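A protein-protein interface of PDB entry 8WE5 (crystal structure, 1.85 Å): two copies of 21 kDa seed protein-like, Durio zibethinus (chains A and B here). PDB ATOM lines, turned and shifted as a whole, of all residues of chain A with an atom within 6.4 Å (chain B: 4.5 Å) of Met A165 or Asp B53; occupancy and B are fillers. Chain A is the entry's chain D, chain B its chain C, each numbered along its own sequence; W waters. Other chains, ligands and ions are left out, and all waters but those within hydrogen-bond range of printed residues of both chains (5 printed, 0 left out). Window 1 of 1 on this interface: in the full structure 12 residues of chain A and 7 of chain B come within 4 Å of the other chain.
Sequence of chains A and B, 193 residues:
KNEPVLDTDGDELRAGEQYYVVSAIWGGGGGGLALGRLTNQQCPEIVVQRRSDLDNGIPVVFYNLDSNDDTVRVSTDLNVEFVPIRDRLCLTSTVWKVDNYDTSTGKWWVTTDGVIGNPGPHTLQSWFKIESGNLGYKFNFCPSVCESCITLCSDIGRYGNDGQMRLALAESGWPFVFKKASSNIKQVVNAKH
Positions printed for both chains: 27 and 29.
Water W5 lies within hydrogen-bond range of the backbone carbonyl oxygen of Gly A28 (2.6 Å), the side-chain carboxylate of Asp B53 (2.7 Å) and the guanidinium group of Arg A158 (2.8 Å). Water W4 lies within hydrogen-bond range of O of Gly B27, O of Trp B26 and N of Gln A164. Water W2 bridges the backbone carbonyl oxygen (O) of Leu B54 (2.7 Å) and the backbone NH (N) of Gly A28 (2.8 Å). Water W1 bridges the backbone carbonyl oxygen (O) of Gly A163 (2.8 Å) and the backbone NH (N) of Trp B26 (2.8 Å). Water W3 lies within hydrogen-bond range of the backbone NH (N) of Met A165, the backbone carbonyl oxygen (O) of Gln A49 and the indole nitrogen (NE1) of Trp B26.
Printed residues of chain B within 4 Å of Gly A28: Trp B26 (3.6 Å), Asp B53 (3.5 Å) and Leu B54 (3.6 Å). Of the printed residues of chain B, Gln A49 touches Trp B26. Of the printed residues of chain B, Gln A164 touches Trp B26 and Gly B27. Met A165 touches three residues of chain B. Of the printed residues of chain A, Gly B27 touches Gly A160 (3.4 Å), Gln A164 (3.8 Å) and Met A165 (3.4 Å). Arg B51 touches none of the printed residues of chain A. The nearest printed residue of chain B that does not touch Gln A49 is Asp B53 (7.2 Å).
Hydrophobic or aromatic side chains of chain A within 4 Å of the printed part of chain B: Met A165. Among the printed residues, 14 pairs touch across the chains.
The backbone NH (N) of Gln A49 lies within hydrogen-bond range of the backbone carbonyl oxygen (O) of Met A165, 2.9 Å away. The side-chain hydroxyl (OG) of Ser B52 sits close to the backbone NH (N) of Leu B54 (3.1 Å). The backbone carbonyl oxygen (O) of Gly A29 lies within hydrogen-bond range of the side-chain amide nitrogen (NE2) of Gln A49, at 2.9 Å. The side-chain amide oxygen (OE1) of Gln A49 lies within hydrogen-bond range of the guanidinium group (NH1) of Arg A158 (2.8 Å). O of Gly A29 sits at hydrogen-bond distance from NH1 of Arg A158 (3.4 Å). The backbone NH of Gly B30 sits at hydrogen-bond distance from the side-chain carboxylate of Asp B53.
Among the printed residues, merely in contact across the chains: Gly A28 with Trp B26 (3.6 Å), Gly A28 with Asp B53 (3.5 Å), Gly A28 with Leu B54 (3.6 Å), Gly A29 with Leu B54 (3.3 Å), Arg A50 with Trp B26 (3.9 Å), Arg A158 with Trp B26 (3.8 Å), Gly A160 with Gly B27 (3.4 Å), Gln A164 with Gly B27 (3.8 Å), Met A165 with Trp B26 (3.3 Å), Met A165 with Gly B27 (3.4 Å) and Met A165 with Asp B53 (3.7 Å).
The backbone carbonyl oxygen (O) of Gly A163 lies close to the backbone carbonyl oxygen (O) of Trp B26 (3.5 Å). The backbone carbonyl oxygen (O) of Trp B26 lies close to the backbone NH (N) of Gln A164 (3.5 Å). NE1 of Trp B26 sits at hydrogen-bond distance from O of Gln A49.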
ATOM      1  N   GLY A  27     -23.691 -12.550  28.774  1.00  0.00           N
ATOM      2  CA  GLY A  27     -22.489 -13.236  28.326  1.00  0.00           C
ATOM      3  C   GLY A  27     -21.972 -12.624  27.041  1.00  0.00           C
ATOM      4  O   GLY A  27     -21.782 -11.405  26.930  1.00  0.00           O
ATOM      5  N   GLY A  28     -21.743 -13.474  26.044  1.00  0.00           N
ATOM      6  CA  GLY A  28     -21.369 -12.938  24.750  1.00  0.00           C
ATOM      7  C   GLY A  28     -22.465 -12.174  24.030  1.00  0.00           C
ATOM      8  O   GLY A  28     -22.217 -11.667  22.934  1.00  0.00           O
ATOM      9  N   GLY A  29     -23.682 -12.113  24.588  1.00  0.00           N
ATOM     10  CA  GLY A  29     -24.743 -11.285  24.043  1.00  0.00           C
ATOM     11  C   GLY A  29     -24.607  -9.795  24.320  1.00  0.00           C
ATOM     12  O   GLY A  29     -25.404  -9.004  23.802  1.00  0.00           O
ATOM     13  N   LEU A  33     -27.167  -0.446  25.379  1.00  0.00           N
ATOM     14  CA  LEU A  33     -26.946   0.414  24.223  1.00  0.00           C
ATOM     15  C   LEU A  33     -26.365   1.763  24.636  1.00  0.00           C
ATOM     16  O   LEU A  33     -26.525   2.209  25.771  1.00  0.00           O
ATOM     17  CB  LEU A  33     -28.239   0.630  23.432  1.00  0.00           C
ATOM     18  CG  LEU A  33     -28.960  -0.633  22.975  1.00  0.00           C
ATOM     19  CD1 LEU A  33     -30.249  -0.263  22.247  1.00  0.00           C
ATOM     20  CD2 LEU A  33     -28.016  -1.405  22.056  1.00  0.00           C
ATOM     21  N   VAL A  47     -25.848   4.403  17.042  1.00  0.00           N
ATOM     22  CA  VAL A  47     -26.294   3.564  18.154  1.00  0.00           C
ATOM     23  C   VAL A  47     -25.428   2.311  18.178  1.00  0.00           C
ATOM     24  O   VAL A  47     -25.341   1.590  17.176  1.00  0.00           O
ATOM     25  CB  VAL A  47     -27.781   3.189  18.026  1.00  0.00           C
ATOM     26  CG1 VAL A  47     -28.204   2.342  19.237  1.00  0.00           C
ATOM     27  CG2 VAL A  47     -28.657   4.440  17.878  1.00  0.00           C
ATOM     28  N   VAL A  48     -24.784   2.042  19.313  1.00  0.00           N
ATOM     29  CA  VAL A  48     -23.904   0.890  19.452  1.00  0.00           C
ATOM     30  C   VAL A  48     -24.293   0.129  20.710  1.00  0.00           C
ATOM     31  O   VAL A  48     -25.049   0.619  21.550  1.00  0.00           O
ATOM     32  CB  VAL A  48     -22.413   1.287  19.526  1.00  0.00           C
ATOM     33  CG1 VAL A  48     -22.006   2.018  18.269  1.00  0.00           C
ATOM     34  CG2 VAL A  48     -22.147   2.145  20.776  1.00  0.00           C
ATOM     35  N   GLN A  49     -23.752  -1.080  20.851  1.00  0.00           N
ATOM     36  CA  GLN A  49     -23.994  -1.870  22.052  1.00  0.00           C
ATOM     37  C   GLN A  49     -22.669  -2.153  22.751  1.00  0.00           C
ATOM     38  O   GLN A  49     -21.698  -2.565  22.099  1.00  0.00           O
ATOM     39  CB  GLN A  49     -24.705  -3.187  21.727  1.00  0.00           C
ATOM     40  CG  GLN A  49     -24.893  -4.051  22.991  1.00  0.00           C
ATOM     41  CD  GLN A  49     -25.239  -5.487  22.681  1.00  0.00           C
ATOM     42  OE1 GLN A  49     -24.880  -6.000  21.621  1.00  0.00           O
ATOM     43  NE2 GLN A  49     -25.853  -6.176  23.650  1.00  0.00           N
ATOM     44  N   ARG A  50     -22.637  -1.928  24.067  1.00  0.00           N
ATOM     45  CA  ARG A  50     -21.464  -2.246  24.875  1.00  0.00           C
ATOM     46  C   ARG A  50     -21.222  -3.752  24.925  1.00  0.00           C
ATOM     47  O   ARG A  50     -22.165  -4.545  24.995  1.00  0.00           O
ATOM     48  CB  ARG A  50     -21.640  -1.702  26.294  1.00  0.00           C
ATOM     49  CG  ARG A  50     -21.891  -0.201  26.318  1.00  0.00           C
ATOM     50  CD  ARG A  50     -20.582   0.573  26.039  1.00  0.00           C
ATOM     51  NE  ARG A  50     -20.685   1.926  26.574  1.00  0.00           N
ATOM     52  CZ  ARG A  50     -20.556   3.034  25.860  1.00  0.00           C
ATOM     53  NH1 ARG A  50     -20.239   2.999  24.575  1.00  0.00           N
ATOM     54  NH2 ARG A  50     -20.766   4.211  26.451  1.00  0.00           N
ATOM     55  N   ARG A 158     -28.648  -6.924  15.372  1.00  0.00           N
ATOM     56  CA  ARG A 158     -27.315  -6.401  15.638  1.00  0.00           C
ATOM     57  C   ARG A 158     -26.375  -6.859  14.536  1.00  0.00           C
ATOM     58  O   ARG A 158     -26.476  -7.994  14.055  1.00  0.00           O
ATOM     59  CB  ARG A 158     -26.771  -6.889  16.994  1.00  0.00           C
ATOM     60  CG  ARG A 158     -27.565  -6.429  18.215  1.00  0.00           C
ATOM     61  CD  ARG A 158     -27.130  -7.162  19.517  1.00  0.00           C
ATOM     62  NE  ARG A 158     -26.855  -8.584  19.324  1.00  0.00           N
ATOM     63  CZ  ARG A 158     -25.786  -9.229  19.779  1.00  0.00           C
ATOM     64  NH1 ARG A 158     -24.863  -8.618  20.512  1.00  0.00           N
ATOM     65  NH2 ARG A 158     -25.659 -10.530  19.522  1.00  0.00           N
ATOM     66  N   TYR A 159     -25.457  -5.979  14.145  1.00  0.00           N
ATOM     67  CA  TYR A 159     -24.469  -6.330  13.137  1.00  0.00           C
ATOM     68  C   TYR A 159     -23.171  -5.611  13.465  1.00  0.00           C
ATOM     69  O   TYR A 159     -23.178  -4.502  14.010  1.00  0.00           O
ATOM     70  CB  TYR A 159     -24.921  -5.936  11.731  1.00  0.00           C
ATOM     71  CG  TYR A 159     -26.028  -6.782  11.156  1.00  0.00           C
ATOM     72  CD1 TYR A 159     -25.794  -8.094  10.780  1.00  0.00           C
ATOM     73  CD2 TYR A 159     -27.307  -6.261  10.984  1.00  0.00           C
ATOM     74  CE1 TYR A 159     -26.799  -8.873  10.250  1.00  0.00           C
ATOM     75  CE2 TYR A 159     -28.327  -7.034  10.439  1.00  0.00           C
ATOM     76  CZ  TYR A 159     -28.059  -8.344  10.080  1.00  0.00           C
ATOM     77  OH  TYR A 159     -29.047  -9.147   9.553  1.00  0.00           O
ATOM     78  N   GLY A 160     -22.057  -6.244  13.108  1.00  0.00           N
ATOM     79  CA  GLY A 160     -20.770  -5.588  13.246  1.00  0.00           C
ATOM     80  C   GLY A 160     -20.559  -4.560  12.144  1.00  0.00           C
ATOM     81  O   GLY A 160     -20.981  -4.740  11.001  1.00  0.00           O
ATOM     82  N   ASN A 161     -19.892  -3.469  12.512  1.00  0.00           N
ATOM     83  CA  ASN A 161     -19.562  -2.375  11.612  1.00  0.00           C
ATOM     84  C   ASN A 161     -18.482  -1.539  12.277  1.00  0.00           C
ATOM     85  O   ASN A 161     -18.626  -1.181  13.447  1.00  0.00           O
ATOM     86  CB  ASN A 161     -20.770  -1.486  11.343  1.00  0.00           C
ATOM     87  CG  ASN A 161     -20.513  -0.455  10.258  1.00  0.00           C
ATOM     88  OD1 ASN A 161     -20.792   0.719  10.459  1.00  0.00           O
ATOM     89  ND2 ASN A 161     -20.071  -0.894   9.086  1.00  0.00           N
ATOM     90  N   GLY A 163     -15.686  -2.029  13.543  1.00  0.00           N
ATOM     91  CA  GLY A 163     -15.162  -2.578  14.780  1.00  0.00           C
ATOM     92  C   GLY A 163     -16.089  -2.491  15.970  1.00  0.00           C
ATOM     93  O   GLY A 163     -15.639  -2.633  17.108  1.00  0.00           O
ATOM     94  N   GLN A 164     -17.382  -2.266  15.748  1.00  0.00           N
ATOM     95  CA  GLN A 164     -18.335  -2.056  16.825  1.00  0.00           C
ATOM     96  C   GLN A 164     -19.569  -2.911  16.563  1.00  0.00           C
ATOM     97  O   GLN A 164     -19.752  -3.448  15.472  1.00  0.00           O
ATOM     98  CB  GLN A 164     -18.727  -0.585  16.929  1.00  0.00           C
ATOM     99  CG  GLN A 164     -17.554   0.320  17.337  1.00  0.00           C
ATOM    100  CD  GLN A 164     -17.901   1.785  17.211  1.00  0.00           C
ATOM    101  OE1 GLN A 164     -18.357   2.388  18.172  1.00  0.00           O
ATOM    102  NE2 GLN A 164     -17.630   2.379  16.041  1.00  0.00           N
ATOM    103  N   MET A 165     -20.427  -3.019  17.577  1.00  0.00           N
ATOM    104  CA  MET A 165     -21.699  -3.733  17.462  1.00  0.00           C
ATOM    105  C   MET A 165     -22.771  -2.659  17.250  1.00  0.00           C
ATOM    106  O   MET A 165     -23.024  -1.858  18.154  1.00  0.00           O
ATOM    107  CB  MET A 165     -22.026  -4.506  18.740  1.00  0.00           C
ATOM    108  CG  MET A 165     -23.284  -5.416  18.591  1.00  0.00           C
ATOM    109  SD  MET A 165     -23.062  -6.786  17.428  1.00  0.00           S
ATOM    110  CE  MET A 165     -21.957  -7.803  18.425  1.00  0.00           C
ATOM    111  N   ARG A 166     -23.401  -2.634  16.075  1.00  0.00           N
ATOM    112  CA  ARG A 166     -24.432  -1.653  15.746  1.00  0.00           C
ATOM    113  C   ARG A 166     -25.805  -2.320  15.689  1.00  0.00           C
ATOM    114  O   ARG A 166     -25.924  -3.541  15.765  1.00  0.00           O
ATOM    115  CB  ARG A 166     -24.133  -0.988  14.395  1.00  0.00           C
ATOM    116  CG  ARG A 166     -22.904  -0.084  14.446  1.00  0.00           C
ATOM    117  CD  ARG A 166     -22.759   0.773  13.188  1.00  0.00           C
ATOM    118  NE  ARG A 166     -23.795   1.798  13.099  1.00  0.00           N
ATOM    119  CZ  ARG A 166     -23.939   2.611  12.059  1.00  0.00           C
ATOM    120  NH1 ARG A 166     -23.071   2.613  11.058  1.00  0.00           N
ATOM    121  NH2 ARG A 166     -24.952   3.471  12.047  1.00  0.00           N
ATOM    122  N   LEU A 167     -26.846  -1.496  15.536  1.00  0.00           N
ATOM    123  CA  LEU A 167     -28.207  -1.957  15.304  1.00  0.00           C
ATOM    124  C   LEU A 167     -28.594  -1.676  13.862  1.00  0.00           C
ATOM    125  O   LEU A 167     -28.279  -0.608  13.332  1.00  0.00           O
ATOM    126  CB  LEU A 167     -29.207  -1.253  16.223  1.00  0.00           C
ATOM    127  CG  LEU A 167     -29.034  -1.478  17.721  1.00  0.00           C
ATOM    128  CD1 LEU A 167     -30.252  -0.905  18.459  1.00  0.00           C
ATOM    129  CD2 LEU A 167     -28.799  -2.939  18.037  1.00  0.00           C
ATOM    130  N   TRP B  26     -15.532  -7.262  18.110  1.00  0.00           N
ATOM    131  CA  TRP B  26     -16.874  -7.137  18.682  1.00  0.00           C
ATOM    132  C   TRP B  26     -17.797  -6.603  17.597  1.00  0.00           C
ATOM    133  O   TRP B  26     -17.625  -5.470  17.134  1.00  0.00           O
ATOM    134  CB  TRP B  26     -16.875  -6.200  19.893  1.00  0.00           C
ATOM    135  CG  TRP B  26     -18.245  -5.955  20.525  1.00  0.00           C
ATOM    136  CD1 TRP B  26     -18.820  -4.747  20.777  1.00  0.00           C
ATOM    137  CD2 TRP B  26     -19.179  -6.948  20.983  1.00  0.00           C
ATOM    138  NE1 TRP B  26     -20.053  -4.915  21.364  1.00  0.00           N
ATOM    139  CE2 TRP B  26     -20.294  -6.257  21.511  1.00  0.00           C
ATOM    140  CE3 TRP B  26     -19.172  -8.348  21.009  1.00  0.00           C
ATOM    141  CZ2 TRP B  26     -21.403  -6.917  22.048  1.00  0.00           C
ATOM    142  CZ3 TRP B  26     -20.276  -9.010  21.547  1.00  0.00           C
ATOM    143  CH2 TRP B  26     -21.374  -8.286  22.067  1.00  0.00           C
ATOM    144  N   GLY B  27     -18.759  -7.424  17.193  1.00  0.00           N
ATOM    145  CA  GLY B  27     -19.560  -7.158  16.024  1.00  0.00           C
ATOM    146  C   GLY B  27     -19.127  -8.035  14.868  1.00  0.00           C
ATOM    147  O   GLY B  27     -18.106  -7.764  14.229  1.00  0.00           O
ATOM    148  N   GLY B  29     -17.846 -10.855  15.089  1.00  0.00           N
ATOM    149  CA  GLY B  29     -16.555 -11.430  15.400  1.00  0.00           C
ATOM    150  C   GLY B  29     -16.581 -12.925  15.669  1.00  0.00           C
ATOM    151  O   GLY B  29     -15.529 -13.562  15.646  1.00  0.00           O
ATOM    152  N   GLY B  30     -17.755 -13.507  15.915  1.00  0.00           N
ATOM    153  CA  GLY B  30     -17.834 -14.918  16.254  1.00  0.00           C
ATOM    154  C   GLY B  30     -17.499 -15.181  17.713  1.00  0.00           C
ATOM    155  O   GLY B  30     -17.185 -14.281  18.491  1.00  0.00           O
ATOM    156  N   GLY B  31     -17.566 -16.451  18.089  1.00  0.00           N
ATOM    157  CA  GLY B  31     -17.340 -16.876  19.463  1.00  0.00           C
ATOM    158  C   GLY B  31     -15.921 -17.346  19.713  1.00  0.00           C
ATOM    159  O   GLY B  31     -14.960 -16.825  19.140  1.00  0.00           O
ATOM    160  N   ARG B  51     -19.368 -19.987  15.482  1.00  0.00           N
ATOM    161  CA  ARG B  51     -20.008 -18.868  14.789  1.00  0.00           C
ATOM    162  C   ARG B  51     -20.758 -17.962  15.757  1.00  0.00           C
ATOM    163  O   ARG B  51     -20.809 -16.741  15.552  1.00  0.00           O
ATOM    164  CB  ARG B  51     -20.972 -19.371  13.698  1.00  0.00           C
ATOM    165  CG  ARG B  51     -21.417 -18.276  12.699  1.00  0.00           C
ATOM    166  CD  ARG B  51     -22.656 -18.684  11.857  1.00  0.00           C
ATOM    167  NE  ARG B  51     -23.844 -18.861  12.692  1.00  0.00           N
ATOM    168  CZ  ARG B  51     -24.523 -17.878  13.273  1.00  0.00           C
ATOM    169  NH1 ARG B  51     -24.279 -16.606  12.996  1.00  0.00           N
ATOM    170  NH2 ARG B  51     -25.458 -18.179  14.169  1.00  0.00           N
ATOM    171  N   SER B  52     -21.356 -18.537  16.797  1.00  0.00           N
ATOM    172  CA  SER B  52     -22.165 -17.775  17.736  1.00  0.00           C
ATOM    173  C   SER B  52     -21.295 -17.042  18.756  1.00  0.00           C
ATOM    174  O   SER B  52     -20.484 -17.666  19.452  1.00  0.00           O
ATOM    175  CB  SER B  52     -23.131 -18.701  18.477  1.00  0.00           C
ATOM    176  OG  SER B  52     -23.712 -17.990  19.556  1.00  0.00           O
ATOM    177  N   ASP B  53     -21.519 -15.724  18.872  1.00  0.00           N
ATOM    178  CA  ASP B  53     -20.890 -14.892  19.905  1.00  0.00           C
ATOM    179  C   ASP B  53     -21.116 -15.429  21.314  1.00  0.00           C
ATOM    180  O   ASP B  53     -20.336 -15.129  22.235  1.00  0.00           O
ATOM    181  CB  ASP B  53     -21.479 -13.478  19.854  1.00  0.00           C
ATOM    182  CG  ASP B  53     -21.025 -12.693  18.654  1.00  0.00           C
ATOM    183  OD1 ASP B  53     -20.334 -13.270  17.791  1.00  0.00           O
ATOM    184  OD2 ASP B  53     -21.428 -11.511  18.542  1.00  0.00           O
ATOM    185  N   LEU B  54     -22.218 -16.146  21.533  1.00  0.00           N
ATOM    186  CA  LEU B  54     -22.540 -16.588  22.881  1.00  0.00           C
ATOM    187  C   LEU B  54     -21.690 -17.753  23.355  1.00  0.00           C
ATOM    188  O   LEU B  54     -21.655 -18.015  24.560  1.00  0.00           O
ATOM    189  CB  LEU B  54     -24.016 -16.995  22.996  1.00  0.00           C
ATOM    190  CG  LEU B  54     -25.029 -16.061  22.349  1.00  0.00           C
ATOM    191  CD1 LEU B  54     -26.446 -16.640  22.542  1.00  0.00           C
ATOM    192  CD2 LEU B  54     -24.890 -14.678  22.984  1.00  0.00           C
ATOM    193  N   ASP B  55     -21.038 -18.459  22.446  1.00  0.00           N
ATOM    194  CA  ASP B  55     -20.330 -19.702  22.743  1.00  0.00           C
ATOM    195  C   ASP B  55     -18.834 -19.409  22.843  1.00  0.00           C
ATOM    196  O   ASP B  55     -18.157 -19.277  21.817  1.00  0.00           O
ATOM    197  CB  ASP B  55     -20.574 -20.737  21.649  1.00  0.00           C
ATOM    198  CG  ASP B  55     -20.261 -22.150  22.100  1.00  0.00           C
ATOM    199  OD1 ASP B  55     -19.285 -22.323  22.865  1.00  0.00           O
ATOM    200  OD2 ASP B  55     -20.861 -23.093  21.547  1.00  0.00           O
HETATM  201  O   HOH W   1     -14.084  -4.851  17.649  1.00  0.00           O
HETATM  202  O   HOH W   2     -22.427 -16.214  26.389  1.00  0.00           O
HETATM  203  O   HOH W   3     -19.940  -1.718  20.039  1.00  0.00           O
HETATM  204  O   HOH W   4     -17.163  -5.285  14.311  1.00  0.00           O
HETATM  205  O   HOH W   5     -23.099 -10.920  20.558  1.00  0.00           O
